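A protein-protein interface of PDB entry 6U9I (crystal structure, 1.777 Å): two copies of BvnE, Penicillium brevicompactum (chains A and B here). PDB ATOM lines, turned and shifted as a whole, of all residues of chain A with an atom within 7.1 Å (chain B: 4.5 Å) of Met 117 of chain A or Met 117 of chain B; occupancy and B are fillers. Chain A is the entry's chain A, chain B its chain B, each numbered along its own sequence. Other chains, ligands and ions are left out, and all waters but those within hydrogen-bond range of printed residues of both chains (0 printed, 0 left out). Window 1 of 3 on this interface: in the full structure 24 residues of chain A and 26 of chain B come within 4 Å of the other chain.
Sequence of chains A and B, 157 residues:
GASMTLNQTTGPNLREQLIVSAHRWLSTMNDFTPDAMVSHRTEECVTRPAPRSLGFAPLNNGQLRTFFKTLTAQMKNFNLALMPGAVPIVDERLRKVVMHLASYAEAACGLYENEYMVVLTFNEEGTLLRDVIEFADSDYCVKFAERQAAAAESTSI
The backbone carbonyl oxygen (O) of Ile 89 of chain A is in hydrogen-bond range of the backbone NH (N) of Val 98 of chain A.
NE2 of His 100 of chain A is in hydrogen-bond range of OE1 of Glu 115 of chain A, at 2.7 Å.
The backbone carbonyl oxygen of Tyr 116 of chain A is in hydrogen-bond range of the backbone NH of Leu 101 of chain A.
O of Phe 135 of chain A is in hydrogen-bond range of N of Met 117 of chain A (2.9 Å).
N of Phe 135 of chain B lies within hydrogen-bond range of O of Met 117 of chain B.
O of Val 119 of chain B sits at hydrogen-bond distance from N of Ile 133 of chain B (2.9 Å).
CG1 of Val 119 of chain B touches CD1 of Ile 89 of chain A, at 3.7 Å.
Val 98 of chain A touches Val 98 of chain B (CG2 to CG2, 3.96 Å).
CE2 of Phe 135 of chain B touches NE2 of His 100 of chain A, 3.8 Å away.
OE1 of Glu 115 of chain A touches CE2 of Phe 135 of chain B, at 3.6 Å.
Phe 135 of chain B touches Tyr 116 of chain A.
Met 117 of chain A touches Met 117 of chain B (CG to CG, 3.5 Å).
CE of Met 117 of chain A touches CD2 of Phe 135 of chain B, 3.8 Å away.
CE2 of Phe 135 of chain A touches NE2 of His 100 of chain B (3.97 Å).
Tyr 116 of chain B touches Phe 135 of chain A.
CD1 of Phe 135 of chain A touches CD1 of Phe 135 of chain B, at 3.7 Å.
Met 117 of chain B touches just these residues of chain A: Met 117 and Phe 135.
Printed residues of chain B within 4 Å of Val 98 of chain A: Val 98 (3.96 Å).
Of the printed residues of chain A, Tyr 116 of chain B touches Phe 135.
Of the printed residues of chain A, His 100 of chain B touches Phe 135.
Of the printed residues of chain A, Val 98 of chain B touches Val 98.
Glu 134 of chain A touches none of the printed residues of chain B.
Ala 50 of chain A touches none of the printed residues of chain B.
Along chain A the printed residues that touch a printed residue of chain B span positions 89 to 136.
Of the 10 printed residues of chain B, 6 touch a printed residue of chain A.
Printed residues of chain B that touch a printed residue of chain A: Val 98, His 100, Tyr 116, Met 117, Val 119 and Phe 135.
Hydrophobic or aromatic side chains of chain B that line the printed part of chain A: Val 98, His 100, Met 117, Val 119 and Phe 135.
Among the printed residues, 12 pairs touch across the chains.
Val 98 of chain A touches its own counterpart, Val 98 of chain B.
His 100 of chain A touches Phe 135 of chain B, and with the chains exchanged Phe 135 of chain A touches His 100 of chain B.
Tyr 116 of chain A touches Phe 135 of chain B, and with the chains exchanged Phe 135 of chain A touches Tyr 116 of chain B.
Phe 135 of chain B touches its own counterpart, Phe 135 of chain A.
Positions printed for both chains: 98, 99, 100, 116, 117, 118, 119, 133, 134 and 135.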
ATOM      1  N   ALA A  50      25.980  -4.277  24.177  1.00  0.00           N
ATOM      2  CA  ALA A  50      26.667  -5.304  24.943  1.00  0.00           C
ATOM      3  C   ALA A  50      26.296  -6.639  24.329  1.00  0.00           C
ATOM      4  O   ALA A  50      25.295  -6.730  23.611  1.00  0.00           O
ATOM      5  CB  ALA A  50      26.279  -5.264  26.431  1.00  0.00           C
ATOM      6  N   ILE A  89      11.152  -5.357  35.119  1.00  0.00           N
ATOM      7  CA  ILE A  89      11.725  -5.483  36.454  1.00  0.00           C
ATOM      8  C   ILE A  89      12.161  -4.087  36.851  1.00  0.00           C
ATOM      9  O   ILE A  89      12.941  -3.468  36.127  1.00  0.00           O
ATOM     10  CB  ILE A  89      12.917  -6.450  36.458  1.00  0.00           C
ATOM     11  CG1 ILE A  89      12.492  -7.807  35.897  1.00  0.00           C
ATOM     12  CG2 ILE A  89      13.503  -6.575  37.854  1.00  0.00           C
ATOM     13  CD1 ILE A  89      13.665  -8.715  35.612  1.00  0.00           C
ATOM     14  N   VAL A  98      14.500  -3.199  33.852  1.00  0.00           N
ATOM     15  CA  VAL A  98      15.129  -4.257  33.061  1.00  0.00           C
ATOM     16  C   VAL A  98      14.043  -5.000  32.292  1.00  0.00           C
ATOM     17  O   VAL A  98      13.004  -5.337  32.866  1.00  0.00           O
ATOM     18  CB  VAL A  98      15.918  -5.221  33.960  1.00  0.00           C
ATOM     19  CG1 VAL A  98      16.539  -6.348  33.130  1.00  0.00           C
ATOM     20  CG2 VAL A  98      17.008  -4.449  34.712  1.00  0.00           C
ATOM     21  N   MET A  99      14.283  -5.261  31.005  1.00  0.00           N
ATOM     22  CA  MET A  99      13.297  -5.955  30.180  1.00  0.00           C
ATOM     23  C   MET A  99      13.969  -6.977  29.279  1.00  0.00           C
ATOM     24  O   MET A  99      14.959  -6.682  28.605  1.00  0.00           O
ATOM     25  CB  MET A  99      12.485  -4.982  29.325  1.00  0.00           C
ATOM     26  CG  MET A  99      11.574  -4.092  30.174  1.00  0.00           C
ATOM     27  SD  MET A  99      10.495  -3.051  29.194  1.00  0.00           S
ATOM     28  CE  MET A  99      11.685  -1.985  28.392  1.00  0.00           C
ATOM     29  N   HIS A 100      13.390  -8.171  29.262  1.00  0.00           N
ATOM     30  CA  HIS A 100      13.789  -9.243  28.363  1.00  0.00           C
ATOM     31  C   HIS A 100      12.924  -9.121  27.113  1.00  0.00           C
ATOM     32  O   HIS A 100      11.704  -9.266  27.193  1.00  0.00           O
ATOM     33  CB  HIS A 100      13.576 -10.577  29.076  1.00  0.00           C
ATOM     34  CG  HIS A 100      14.185 -11.754  28.388  1.00  0.00           C
ATOM     35  ND1 HIS A 100      13.864 -13.049  28.736  1.00  0.00           N
ATOM     36  CD2 HIS A 100      15.092 -11.843  27.384  1.00  0.00           C
ATOM     37  CE1 HIS A 100      14.545 -13.889  27.973  1.00  0.00           C
ATOM     38  NE2 HIS A 100      15.298 -13.183  27.145  1.00  0.00           N
ATOM     39  N   LEU A 101      13.545  -8.830  25.967  1.00  0.00           N
ATOM     40  CA  LEU A 101      12.828  -8.391  24.775  1.00  0.00           C
ATOM     41  C   LEU A 101      13.130  -9.278  23.578  1.00  0.00           C
ATOM     42  O   LEU A 101      14.222  -9.834  23.450  1.00  0.00           O
ATOM     43  CB  LEU A 101      13.199  -6.949  24.388  1.00  0.00           C
ATOM     44  CG  LEU A 101      12.972  -5.847  25.424  1.00  0.00           C
ATOM     45  CD1 LEU A 101      13.442  -4.492  24.880  1.00  0.00           C
ATOM     46  CD2 LEU A 101      11.513  -5.770  25.872  1.00  0.00           C
ATOM     47  N   GLU A 115      17.035 -11.155  20.241  1.00  0.00           N
ATOM     48  CA  GLU A 115      16.624 -11.264  21.634  1.00  0.00           C
ATOM     49  C   GLU A 115      17.599 -10.460  22.476  1.00  0.00           C
ATOM     50  O   GLU A 115      18.811 -10.503  22.232  1.00  0.00           O
ATOM     51  CB  GLU A 115      16.606 -12.731  22.091  1.00  0.00           C
ATOM     52  CG  GLU A 115      16.187 -12.945  23.544  1.00  0.00           C
ATOM     53  CD  GLU A 115      16.285 -14.405  23.969  1.00  0.00           C
ATOM     54  OE1 GLU A 115      16.300 -14.681  25.192  1.00  0.00           O
ATOM     55  OE2 GLU A 115      16.344 -15.284  23.076  1.00  0.00           O
ATOM     56  N   TYR A 116      17.082  -9.721  23.457  1.00  0.00           N
ATOM     57  CA  TYR A 116      17.921  -8.812  24.229  1.00  0.00           C
ATOM     58  C   TYR A 116      17.525  -8.824  25.693  1.00  0.00           C
ATOM     59  O   TYR A 116      16.366  -9.064  26.039  1.00  0.00           O
ATOM     60  CB  TYR A 116      17.827  -7.353  23.762  1.00  0.00           C
ATOM     61  CG  TYR A 116      17.680  -7.164  22.282  1.00  0.00           C
ATOM     62  CD1 TYR A 116      16.453  -7.392  21.660  1.00  0.00           C
ATOM     63  CD2 TYR A 116      18.750  -6.745  21.502  1.00  0.00           C
ATOM     64  CE1 TYR A 116      16.303  -7.222  20.317  1.00  0.00           C
ATOM     65  CE2 TYR A 116      18.602  -6.575  20.130  1.00  0.00           C
ATOM     66  CZ  TYR A 116      17.379  -6.812  19.553  1.00  0.00           C
ATOM     67  OH  TYR A 116      17.189  -6.644  18.191  1.00  0.00           O
ATOM     68  N   MET A 117      18.493  -8.499  26.541  1.00  0.00           N
ATOM     69  CA  MET A 117      18.232  -8.025  27.894  1.00  0.00           C
ATOM     70  C   MET A 117      18.632  -6.557  27.930  1.00  0.00           C
ATOM     71  O   MET A 117      19.802  -6.222  27.703  1.00  0.00           O
ATOM     72  CB  MET A 117      19.007  -8.842  28.931  1.00  0.00           C
ATOM     73  CG  MET A 117      18.501  -8.703  30.358  1.00  0.00           C
ATOM     74  SD  MET A 117      16.878  -9.465  30.625  1.00  0.00           S
ATOM     75  CE  MET A 117      17.226 -11.194  30.345  1.00  0.00           C
ATOM     76  N   VAL A 118      17.668  -5.679  28.202  1.00  0.00           N
ATOM     77  CA  VAL A 118      17.876  -4.235  28.177  1.00  0.00           C
ATOM     78  C   VAL A 118      17.777  -3.690  29.596  1.00  0.00           C
ATOM     79  O   VAL A 118      16.919  -4.117  30.378  1.00  0.00           O
ATOM     80  CB  VAL A 118      16.847  -3.571  27.234  1.00  0.00           C
ATOM     81  CG1 VAL A 118      16.756  -2.074  27.460  1.00  0.00           C
ATOM     82  CG2 VAL A 118      17.203  -3.889  25.779  1.00  0.00           C
ATOM     83  N   VAL A 119      18.667  -2.754  29.936  1.00  0.00           N
ATOM     84  CA  VAL A 119      18.617  -2.040  31.210  1.00  0.00           C
ATOM     85  C   VAL A 119      18.431  -0.563  30.885  1.00  0.00           C
ATOM     86  O   VAL A 119      19.343   0.076  30.345  1.00  0.00           O
ATOM     87  CB  VAL A 119      19.879  -2.249  32.054  1.00  0.00           C
ATOM     88  CG1 VAL A 119      19.743  -1.494  33.389  1.00  0.00           C
ATOM     89  CG2 VAL A 119      20.155  -3.743  32.268  1.00  0.00           C
ATOM     90  N   ILE A 133      21.516   0.085  28.398  1.00  0.00           N
ATOM     91  CA  ILE A 133      22.383  -1.026  28.018  1.00  0.00           C
ATOM     92  C   ILE A 133      21.543  -1.996  27.218  1.00  0.00           C
ATOM     93  O   ILE A 133      20.481  -2.421  27.686  1.00  0.00           O
ATOM     94  CB  ILE A 133      22.972  -1.753  29.231  1.00  0.00           C
ATOM     95  CG1 ILE A 133      23.775  -0.809  30.100  1.00  0.00           C
ATOM     96  CG2 ILE A 133      23.812  -2.962  28.752  1.00  0.00           C
ATOM     97  CD1 ILE A 133      24.147  -1.457  31.404  1.00  0.00           C
ATOM     98  N   GLU A 134      22.011  -2.361  26.033  1.00  0.00           N
ATOM     99  CA  GLU A 134      21.300  -3.303  25.170  1.00  0.00           C
ATOM    100  C   GLU A 134      22.172  -4.543  25.008  1.00  0.00           C
ATOM    101  O   GLU A 134      23.080  -4.574  24.172  1.00  0.00           O
ATOM    102  CB  GLU A 134      20.957  -2.665  23.827  1.00  0.00           C
ATOM    103  CG  GLU A 134      19.903  -1.585  23.942  1.00  0.00           C
ATOM    104  CD  GLU A 134      19.635  -0.869  22.635  1.00  0.00           C
ATOM    105  OE1 GLU A 134      20.413  -1.054  21.673  1.00  0.00           O
ATOM    106  OE2 GLU A 134      18.641  -0.113  22.574  1.00  0.00           O
ATOM    107  N   PHE A 135      21.889  -5.572  25.808  1.00  0.00           N
ATOM    108  CA  PHE A 135      22.661  -6.815  25.788  1.00  0.00           C
ATOM    109  C   PHE A 135      21.995  -7.766  24.793  1.00  0.00           C
ATOM    110  O   PHE A 135      20.955  -8.358  25.092  1.00  0.00           O
ATOM    111  CB  PHE A 135      22.714  -7.410  27.195  1.00  0.00           C
ATOM    112  CG  PHE A 135      23.784  -8.461  27.388  1.00  0.00           C
ATOM    113  CD1 PHE A 135      23.664  -9.713  26.795  1.00  0.00           C
ATOM    114  CD2 PHE A 135      24.880  -8.209  28.203  1.00  0.00           C
ATOM    115  CE1 PHE A 135      24.643 -10.696  26.976  1.00  0.00           C
ATOM    116  CE2 PHE A 135      25.868  -9.193  28.394  1.00  0.00           C
ATOM    117  CZ  PHE A 135      25.752 -10.425  27.775  1.00  0.00           C
ATOM    118  N   ALA A 136      22.596  -7.918  23.617  1.00  0.00           N
ATOM    119  CA  ALA A 136      22.007  -8.661  22.511  1.00  0.00           C
ATOM    120  C   ALA A 136      22.449 -10.123  22.510  1.00  0.00           C
ATOM    121  O   ALA A 136      23.425 -10.513  23.161  1.00  0.00           O
ATOM    122  CB  ALA A 136      22.386  -8.016  21.169  1.00  0.00           C
ATOM    123  N   ASP A 137      21.691 -10.938  21.772  1.00  0.00           N
ATOM    124  CA  ASP A 137      22.115 -12.272  21.341  1.00  0.00           C
ATOM    125  C   ASP A 137      23.250 -12.072  20.339  1.00  0.00           C
ATOM    126  O   ASP A 137      23.015 -11.754  19.170  1.00  0.00           O
ATOM    127  CB  ASP A 137      20.920 -13.004  20.727  1.00  0.00           C
ATOM    128  CG  ASP A 137      21.245 -14.420  20.231  1.00  0.00           C
ATOM    129  OD1 ASP A 137      22.421 -14.786  20.018  1.00  0.00           O
ATOM    130  OD2 ASP A 137      20.280 -15.177  20.015  1.00  0.00           O
ATOM    131  N   VAL B  98      19.017  -8.207  39.356  1.00  0.00           N
ATOM    132  CA  VAL B  98      19.659  -8.307  38.052  1.00  0.00           C
ATOM    133  C   VAL B  98      21.119  -7.930  38.231  1.00  0.00           C
ATOM    134  O   VAL B  98      21.424  -6.941  38.905  1.00  0.00           O
ATOM    135  CB  VAL B  98      18.984  -7.389  37.014  1.00  0.00           C
ATOM    136  CG1 VAL B  98      19.653  -7.533  35.648  1.00  0.00           C
ATOM    137  CG2 VAL B  98      17.492  -7.701  36.913  1.00  0.00           C
ATOM    138  N   MET B  99      22.015  -8.715  37.645  1.00  0.00           N
ATOM    139  CA  MET B  99      23.438  -8.424  37.741  1.00  0.00           C
ATOM    140  C   MET B  99      24.119  -8.664  36.407  1.00  0.00           C
ATOM    141  O   MET B  99      23.825  -9.642  35.714  1.00  0.00           O
ATOM    142  CB  MET B  99      24.112  -9.284  38.819  1.00  0.00           C
ATOM    143  CG  MET B  99      23.629  -8.983  40.231  1.00  0.00           C
ATOM    144  SD  MET B  99      24.593  -9.915  41.446  1.00  0.00           S
ATOM    145  CE  MET B  99      23.889 -11.542  41.218  1.00  0.00           C
ATOM    146  N   HIS B 100      25.072  -7.788  36.088  1.00  0.00           N
ATOM    147  CA  HIS B 100      25.902  -7.870  34.896  1.00  0.00           C
ATOM    148  C   HIS B 100      27.244  -8.474  35.310  1.00  0.00           C
ATOM    149  O   HIS B 100      27.976  -7.869  36.097  1.00  0.00           O
ATOM    150  CB  HIS B 100      26.067  -6.458  34.321  1.00  0.00           C
ATOM    151  CG  HIS B 100      26.728  -6.396  32.983  1.00  0.00           C
ATOM    152  ND1 HIS B 100      27.278  -5.231  32.490  1.00  0.00           N
ATOM    153  CD2 HIS B 100      26.928  -7.340  32.033  1.00  0.00           C
ATOM    154  CE1 HIS B 100      27.795  -5.462  31.295  1.00  0.00           C
ATOM    155  NE2 HIS B 100      27.596  -6.736  30.995  1.00  0.00           N
ATOM    156  N   TYR B 116      27.646 -11.963  31.020  1.00  0.00           N
ATOM    157  CA  TYR B 116      26.260 -12.360  31.260  1.00  0.00           C
ATOM    158  C   TYR B 116      25.442 -11.209  31.804  1.00  0.00           C
ATOM    159  O   TYR B 116      25.941 -10.352  32.531  1.00  0.00           O
ATOM    160  CB  TYR B 116      26.124 -13.508  32.281  1.00  0.00           C
ATOM    161  CG  TYR B 116      27.067 -14.648  32.035  1.00  0.00           C
ATOM    162  CD1 TYR B 116      28.402 -14.549  32.401  1.00  0.00           C
ATOM    163  CD2 TYR B 116      26.638 -15.804  31.406  1.00  0.00           C
ATOM    164  CE1 TYR B 116      29.276 -15.560  32.156  1.00  0.00           C
ATOM    165  CE2 TYR B 116      27.523 -16.846  31.168  1.00  0.00           C
ATOM    166  CZ  TYR B 116      28.846 -16.706  31.545  1.00  0.00           C
ATOM    167  OH  TYR B 116      29.763 -17.704  31.315  1.00  0.00           O
ATOM    168  N   MET B 117      24.153 -11.240  31.488  1.00  0.00           N
ATOM    169  CA  MET B 117      23.139 -10.526  32.249  1.00  0.00           C
ATOM    170  C   MET B 117      22.314 -11.603  32.946  1.00  0.00           C
ATOM    171  O   MET B 117      21.811 -12.523  32.288  1.00  0.00           O
ATOM    172  CB  MET B 117      22.281  -9.644  31.333  1.00  0.00           C
ATOM    173  CG  MET B 117      21.593  -8.478  32.022  1.00  0.00           C
ATOM    174  SD  MET B 117      22.725  -7.249  32.715  1.00  0.00           S
ATOM    175  CE  MET B 117      23.327  -6.382  31.272  1.00  0.00           C
ATOM    176  N   VAL B 118      22.220 -11.535  34.266  1.00  0.00           N
ATOM    177  CA  VAL B 118      21.562 -12.570  35.053  1.00  0.00           C
ATOM    178  C   VAL B 118      20.373 -11.967  35.788  1.00  0.00           C
ATOM    179  O   VAL B 118      20.473 -10.871  36.353  1.00  0.00           O
ATOM    180  CB  VAL B 118      22.564 -13.214  36.035  1.00  0.00           C
ATOM    181  CG1 VAL B 118      21.852 -14.035  37.078  1.00  0.00           C
ATOM    182  CG2 VAL B 118      23.571 -14.063  35.261  1.00  0.00           C
ATOM    183  N   VAL B 119      19.243 -12.673  35.771  1.00  0.00           N
ATOM    184  CA  VAL B 119      18.056 -12.276  36.531  1.00  0.00           C
ATOM    185  C   VAL B 119      17.806 -13.349  37.577  1.00  0.00           C
ATOM    186  O   VAL B 119      17.508 -14.499  37.228  1.00  0.00           O
ATOM    187  CB  VAL B 119      16.817 -12.096  35.645  1.00  0.00           C
ATOM    188  CG1 VAL B 119      15.634 -11.669  36.505  1.00  0.00           C
ATOM    189  CG2 VAL B 119      17.077 -11.086  34.532  1.00  0.00           C
ATOM    190  N   ILE B 133      17.525 -16.554  35.239  1.00  0.00           N
ATOM    191  CA  ILE B 133      17.776 -16.392  33.813  1.00  0.00           C
ATOM    192  C   ILE B 133      19.251 -16.063  33.665  1.00  0.00           C
ATOM    193  O   ILE B 133      19.733 -15.088  34.247  1.00  0.00           O
ATOM    194  CB  ILE B 133      16.914 -15.283  33.197  1.00  0.00           C
ATOM    195  CG1 ILE B 133      15.430 -15.614  33.321  1.00  0.00           C
ATOM    196  CG2 ILE B 133      17.308 -15.056  31.731  1.00  0.00           C
ATOM    197  CD1 ILE B 133      14.565 -14.458  32.883  1.00  0.00           C
ATOM    198  N   GLU B 134      19.968 -16.879  32.910  1.00  0.00           N
ATOM    199  CA  GLU B 134      21.401 -16.711  32.691  1.00  0.00           C
ATOM    200  C   GLU B 134      21.576 -16.379  31.209  1.00  0.00           C
ATOM    201  O   GLU B 134      21.631 -17.272  30.363  1.00  0.00           O
ATOM    202  CB  GLU B 134      22.148 -17.989  33.111  1.00  0.00           C
ATOM    203  CG  GLU B 134      23.606 -18.049  32.709  1.00  0.00           C
ATOM    204  CD  GLU B 134      24.229 -19.417  32.988  1.00  0.00           C
ATOM    205  OE1 GLU B 134      23.767 -20.109  33.929  1.00  0.00           O
ATOM    206  OE2 GLU B 134      25.171 -19.800  32.256  1.00  0.00           O
ATOM    207  N   PHE B 135      21.634 -15.077  30.899  1.00  0.00           N
ATOM    208  CA  PHE B 135      21.709 -14.599  29.515  1.00  0.00           C
ATOM    209  C   PHE B 135      23.184 -14.397  29.174  1.00  0.00           C
ATOM    210  O   PHE B 135      23.796 -13.398  29.558  1.00  0.00           O
ATOM    211  CB  PHE B 135      20.878 -13.325  29.358  1.00  0.00           C
ATOM    212  CG  PHE B 135      20.551 -12.946  27.927  1.00  0.00           C
ATOM    213  CD1 PHE B 135      21.548 -12.717  26.994  1.00  0.00           C
ATOM    214  CD2 PHE B 135      19.231 -12.758  27.539  1.00  0.00           C
ATOM    215  CE1 PHE B 135      21.231 -12.331  25.683  1.00  0.00           C
ATOM    216  CE2 PHE B 135      18.901 -12.363  26.235  1.00  0.00           C
ATOM    217  CZ  PHE B 135      19.905 -12.155  25.303  1.00  0.00           C
